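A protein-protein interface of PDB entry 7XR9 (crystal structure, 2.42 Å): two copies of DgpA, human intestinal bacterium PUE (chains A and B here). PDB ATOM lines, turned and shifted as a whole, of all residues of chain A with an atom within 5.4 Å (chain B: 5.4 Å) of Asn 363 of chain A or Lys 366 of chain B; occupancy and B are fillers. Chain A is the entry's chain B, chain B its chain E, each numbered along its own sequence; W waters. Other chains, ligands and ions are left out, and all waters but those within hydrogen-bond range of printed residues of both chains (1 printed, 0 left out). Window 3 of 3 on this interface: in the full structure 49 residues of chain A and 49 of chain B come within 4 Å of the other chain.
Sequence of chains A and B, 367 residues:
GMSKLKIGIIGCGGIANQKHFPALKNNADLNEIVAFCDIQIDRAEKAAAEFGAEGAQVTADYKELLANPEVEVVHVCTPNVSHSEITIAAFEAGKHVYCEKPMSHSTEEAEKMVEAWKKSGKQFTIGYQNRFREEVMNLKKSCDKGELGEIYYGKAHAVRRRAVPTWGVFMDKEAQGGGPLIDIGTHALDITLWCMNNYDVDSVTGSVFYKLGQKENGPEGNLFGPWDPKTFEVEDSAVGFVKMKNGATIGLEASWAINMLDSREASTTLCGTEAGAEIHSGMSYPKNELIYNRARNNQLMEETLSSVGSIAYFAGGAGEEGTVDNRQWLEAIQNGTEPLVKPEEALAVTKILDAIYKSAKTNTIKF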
ATOM      1  N   VAL A 204      14.734 -21.816  26.972  1.00  0.00           N
ATOM      2  CA  VAL A 204      15.826 -21.680  27.921  1.00  0.00           C
ATOM      3  C   VAL A 204      17.105 -22.152  27.240  1.00  0.00           C
ATOM      4  O   VAL A 204      17.113 -23.208  26.601  1.00  0.00           O
ATOM      5  CB  VAL A 204      15.557 -22.498  29.197  1.00  0.00           C
ATOM      6  CG1 VAL A 204      16.719 -22.394  30.148  1.00  0.00           C
ATOM      7  CG2 VAL A 204      14.274 -22.037  29.863  1.00  0.00           C
ATOM      8  N   THR A 205      18.177 -21.373  27.355  1.00  0.00           N
ATOM      9  CA  THR A 205      19.473 -21.750  26.803  1.00  0.00           C
ATOM     10  C   THR A 205      20.524 -21.484  27.867  1.00  0.00           C
ATOM     11  O   THR A 205      20.555 -20.394  28.444  1.00  0.00           O
ATOM     12  CB  THR A 205      19.811 -20.967  25.518  1.00  0.00           C
ATOM     13  OG1 THR A 205      18.685 -20.951  24.635  1.00  0.00           O
ATOM     14  CG2 THR A 205      21.006 -21.599  24.800  1.00  0.00           C
ATOM     15  N   LYS A 358      19.970 -28.780  31.311  1.00  0.00           N
ATOM     16  CA  LYS A 358      19.681 -29.683  30.165  1.00  0.00           C
ATOM     17  C   LYS A 358      20.329 -29.121  28.905  1.00  0.00           C
ATOM     18  O   LYS A 358      20.627 -29.905  28.019  1.00  0.00           O
ATOM     19  CB  LYS A 358      18.177 -29.927  30.023  1.00  0.00           C
ATOM     20  CG  LYS A 358      17.765 -31.068  29.104  1.00  0.00           C
ATOM     21  CD  LYS A 358      16.263 -31.173  28.954  1.00  0.00           C
ATOM     22  CE  LYS A 358      15.801 -32.443  28.275  1.00  0.00           C
ATOM     23  NZ  LYS A 358      16.271 -32.527  26.873  1.00  0.00           N
ATOM     24  N   SER A 359      20.559 -27.819  28.842  1.00  0.00           N
ATOM     25  CA  SER A 359      21.342 -27.300  27.701  1.00  0.00           C
ATOM     26  C   SER A 359      22.771 -27.848  27.833  1.00  0.00           C
ATOM     27  O   SER A 359      23.703 -27.108  27.506  1.00  0.00           O
ATOM     28  CB  SER A 359      21.249 -25.808  27.609  1.00  0.00           C
ATOM     29  N   LYS A 361      23.071 -30.347  26.383  1.00  0.00           N
ATOM     30  CA  LYS A 361      22.805 -31.062  25.137  1.00  0.00           C
ATOM     31  C   LYS A 361      23.136 -30.072  24.029  1.00  0.00           C
ATOM     32  O   LYS A 361      22.814 -30.372  22.885  1.00  0.00           O
ATOM     33  CB  LYS A 361      21.355 -31.414  25.160  1.00  0.00           C
ATOM     34  N   THR A 362      23.792 -28.964  24.374  1.00  0.00           N
ATOM     35  CA  THR A 362      24.064 -27.863  23.413  1.00  0.00           C
ATOM     36  C   THR A 362      22.796 -27.689  22.584  1.00  0.00           C
ATOM     37  O   THR A 362      22.888 -27.549  21.364  1.00  0.00           O
ATOM     38  CB  THR A 362      25.384 -28.026  22.651  1.00  0.00           C
ATOM     39  OG1 THR A 362      25.681 -26.764  22.055  1.00  0.00           O
ATOM     40  CG2 THR A 362      25.351 -29.109  21.597  1.00  0.00           C
ATOM     41  N   ASN A 363      21.662 -27.688  23.267  1.00  0.00           N
ATOM     42  CA  ASN A 363      20.381 -27.449  22.571  1.00  0.00           C
ATOM     43  C   ASN A 363      19.484 -26.552  23.428  1.00  0.00           C
ATOM     44  O   ASN A 363      19.435 -26.763  24.640  1.00  0.00           O
ATOM     45  CB  ASN A 363      19.724 -28.760  22.139  1.00  0.00           C
ATOM     46  CG  ASN A 363      19.847 -29.021  20.654  1.00  0.00           C
ATOM     47  OD1 ASN A 363      19.304 -28.278  19.840  1.00  0.00           O
ATOM     48  ND2 ASN A 363      20.546 -30.082  20.289  1.00  0.00           N
ATOM     49  N   THR A 364      18.853 -25.559  22.815  1.00  0.00           N
ATOM     50  CA  THR A 364      17.875 -24.678  23.477  1.00  0.00           C
ATOM     51  C   THR A 364      16.653 -25.520  23.803  1.00  0.00           C
ATOM     52  O   THR A 364      16.276 -26.282  22.983  1.00  0.00           O
ATOM     53  CB  THR A 364      17.514 -23.512  22.564  1.00  0.00           C
ATOM     54  OG1 THR A 364      18.653 -22.690  22.351  1.00  0.00           O
ATOM     55  CG2 THR A 364      16.373 -22.696  23.117  1.00  0.00           C
ATOM     56  N   ILE A 365      16.090 -25.364  24.975  1.00  0.00           N
ATOM     57  CA  ILE A 365      14.913 -26.138  25.423  1.00  0.00           C
ATOM     58  C   ILE A 365      13.653 -25.311  25.225  1.00  0.00           C
ATOM     59  O   ILE A 365      13.524 -24.299  25.818  1.00  0.00           O
ATOM     60  CB  ILE A 365      15.075 -26.616  26.875  1.00  0.00           C
ATOM     61  CG1 ILE A 365      16.462 -27.190  27.133  1.00  0.00           C
ATOM     62  CG2 ILE A 365      13.990 -27.595  27.255  1.00  0.00           C
ATOM     63  CD1 ILE A 365      16.726 -28.457  26.401  1.00  0.00           C
ATOM     64  N   ASP B 202      29.236 -21.600  17.848  1.00  0.00           N
ATOM     65  CA  ASP B 202      28.399 -22.784  17.694  1.00  0.00           C
ATOM     66  C   ASP B 202      26.915 -22.464  17.731  1.00  0.00           C
ATOM     67  O   ASP B 202      26.172 -22.938  16.866  1.00  0.00           O
ATOM     68  CB  ASP B 202      28.720 -23.847  18.756  1.00  0.00           C
ATOM     69  CG  ASP B 202      28.091 -25.197  18.427  1.00  0.00           C
ATOM     70  OD1 ASP B 202      28.672 -25.871  17.559  1.00  0.00           O
ATOM     71  OD2 ASP B 202      27.048 -25.586  19.013  1.00  0.00           O
ATOM     72  N   SER B 203      26.415 -21.574  18.586  1.00  0.00           N
ATOM     73  CA  SER B 203      25.022 -21.173  18.497  1.00  0.00           C
ATOM     74  C   SER B 203      24.875 -19.735  18.956  1.00  0.00           C
ATOM     75  O   SER B 203      25.685 -19.231  19.737  1.00  0.00           O
ATOM     76  CB  SER B 203      24.093 -22.090  19.312  1.00  0.00           C
ATOM     77  OG  SER B 203      24.447 -22.133  20.685  1.00  0.00           O
ATOM     78  N   VAL B 204      23.817 -19.093  18.458  1.00  0.00           N
ATOM     79  CA  VAL B 204      23.484 -17.704  18.745  1.00  0.00           C
ATOM     80  C   VAL B 204      21.986 -17.627  19.026  1.00  0.00           C
ATOM     81  O   VAL B 204      21.172 -17.948  18.153  1.00  0.00           O
ATOM     82  CB  VAL B 204      23.846 -16.768  17.578  1.00  0.00           C
ATOM     83  CG1 VAL B 204      23.419 -15.355  17.889  1.00  0.00           C
ATOM     84  CG2 VAL B 204      25.334 -16.826  17.279  1.00  0.00           C
ATOM     85  N   LYS B 243      27.209 -18.975  22.182  1.00  0.00           N
ATOM     86  CA  LYS B 243      27.970 -20.128  22.696  1.00  0.00           C
ATOM     87  C   LYS B 243      29.024 -20.469  21.647  1.00  0.00           C
ATOM     88  O   LYS B 243      28.697 -20.498  20.463  1.00  0.00           O
ATOM     89  CB  LYS B 243      27.009 -21.281  22.991  1.00  0.00           C
ATOM     90  CG  LYS B 243      25.984 -21.011  24.081  1.00  0.00           C
ATOM     91  CD  LYS B 243      25.152 -22.219  24.425  1.00  0.00           C
ATOM     92  CE  LYS B 243      25.944 -23.319  25.096  1.00  0.00           C
ATOM     93  NZ  LYS B 243      25.054 -24.376  25.626  1.00  0.00           N
ATOM     94  N   THR B 364      17.023 -20.446  17.890  1.00  0.00           N
ATOM     95  CA  THR B 364      18.469 -20.392  18.032  1.00  0.00           C
ATOM     96  C   THR B 364      19.110 -20.701  16.687  1.00  0.00           C
ATOM     97  O   THR B 364      18.712 -21.655  16.010  1.00  0.00           O
ATOM     98  CB  THR B 364      18.943 -21.399  19.083  1.00  0.00           C
ATOM     99  OG1 THR B 364      18.370 -21.069  20.353  1.00  0.00           O
ATOM    100  CG2 THR B 364      20.468 -21.396  19.193  1.00  0.00           C
ATOM    101  N   ILE B 365      20.096 -19.901  16.299  1.00  0.00           N
ATOM    102  CA  ILE B 365      20.837 -20.140  15.064  1.00  0.00           C
ATOM    103  C   ILE B 365      22.059 -21.000  15.366  1.00  0.00           C
ATOM    104  O   ILE B 365      22.981 -20.570  16.069  1.00  0.00           O
ATOM    105  CB  ILE B 365      21.245 -18.824  14.394  1.00  0.00           C
ATOM    106  CG1 ILE B 365      20.050 -18.216  13.663  1.00  0.00           C
ATOM    107  CG2 ILE B 365      22.367 -19.075  13.408  1.00  0.00           C
ATOM    108  CD1 ILE B 365      18.885 -17.955  14.554  1.00  0.00           C
ATOM    109  N   LYS B 366      22.072 -22.212  14.823  1.00  0.00           N
ATOM    110  CA  LYS B 366      23.264 -23.034  14.967  1.00  0.00           C
ATOM    111  C   LYS B 366      24.231 -22.747  13.828  1.00  0.00           C
ATOM    112  O   LYS B 366      23.822 -22.599  12.676  1.00  0.00           O
ATOM    113  CB  LYS B 366      22.894 -24.517  14.999  1.00  0.00           C
ATOM    114  CG  LYS B 366      22.517 -25.023  16.397  1.00  0.00           C
ATOM    115  CD  LYS B 366      21.231 -25.839  16.393  1.00  0.00           C
ATOM    116  CE  LYS B 366      21.345 -27.023  17.346  1.00  0.00           C
ATOM    117  NZ  LYS B 366      20.399 -28.119  16.998  1.00  0.00           N
ATOM    118  N   PHE B 367      25.508 -22.706  14.193  1.00  0.00           N
ATOM    119  CA  PHE B 367      26.574 -22.445  13.229  1.00  0.00           C
ATOM    120  C   PHE B 367      27.330 -23.736  12.911  1.00  0.00           C
ATOM    121  O   PHE B 367      28.090 -23.803  11.945  1.00  0.00           O
ATOM    122  CB  PHE B 367      27.548 -21.390  13.765  1.00  0.00           C
ATOM    123  CG  PHE B 367      27.045 -19.976  13.659  1.00  0.00           C
ATOM    124  CD1 PHE B 367      25.785 -19.635  14.122  1.00  0.00           C
ATOM    125  CD2 PHE B 367      27.851 -18.979  13.118  1.00  0.00           C
ATOM    126  CE1 PHE B 367      25.327 -18.338  14.036  1.00  0.00           C
ATOM    127  CE2 PHE B 367      27.405 -17.679  13.031  1.00  0.00           C
ATOM    128  CZ  PHE B 367      26.139 -17.356  13.489  1.00  0.00           C
HETATM  129  O   HOH W   1      22.835 -24.645  24.061  1.00  0.00           O
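The side-chain amino group (NZ) of Lys 366 of chain B lies within hydrogen-bond range of the side-chain amide oxygen (OD1) of Asn 363 of chain A, 3.0 Å away.
OG1 of Thr 364 of chain A is in hydrogen-bond range of OG1 of Thr 364 of chain B (2.6 Å).
The side-chain hydroxyl (OG1) of Thr 205 of chain A sits at hydrogen-bond distance from the side-chain hydroxyl (OG1) of Thr 364 of chain A, at 2.9 Å.
N of Asp 202 of chain B sits at hydrogen-bond distance from O of Lys 243 of chain B (2.9 Å).
The backbone carbonyl oxygen (O) of Asp 202 of chain B lies within hydrogen-bond range of the backbone NH (N) of Phe 367 of chain B (2.8 Å).
The side-chain amide nitrogen of Asn 363 of chain A is in hydrogen-bond range of the backbone carbonyl oxygen of Lys 361 of chain A (3.5 Å).
The backbone carbonyl oxygen (O) of Ser 203 of chain B lies within hydrogen-bond range of the backbone NH (N) of Lys 243 of chain B, at 2.9 Å.
Among the printed residues, pairs that only touch across the chains: Ser 359 of chain A with Lys 243 of chain B (3.6 Å) and Thr 362 of chain A with Asp 202 of chain B (3.5 Å).
Of the printed residues of chain B, Ser 359 of chain A touches Lys 243.
Printed residues of chain B within 4 Å of Thr 362 of chain A: Asp 202 (3.5 Å).
Of chain B, only Lys 366 comes within 4 Å of Asn 363 of chain A.
Of the printed residues of chain B, Thr 364 of chain A touches Thr 364 (2.6 Å).
Of the printed residues of chain A, Lys 243 of chain B touches Ser 359 (3.6 Å).
Of the printed residues of chain A, Lys 366 of chain B touches Asn 363 (3.0 Å).
The nearest residue of chain A that does not touch Lys 366 of chain B is Thr 362 of chain A (4.3 Å).
The nearest printed residue of chain B that does not touch Thr 364 of chain A is Ser 203 of chain B (6.1 Å).
Of the 9 printed residues of chain A, 4 touch a printed residue of chain B.
Of the 8 printed residues of chain B, 4 touch a printed residue of chain A.
Thr 364 of chain A touches its own counterpart, Thr 364 of chain B.
3 positions are printed for both chains.
Water W1 bridges NZ of Lys 243 of chain B and N of Asn 363 of chain A.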
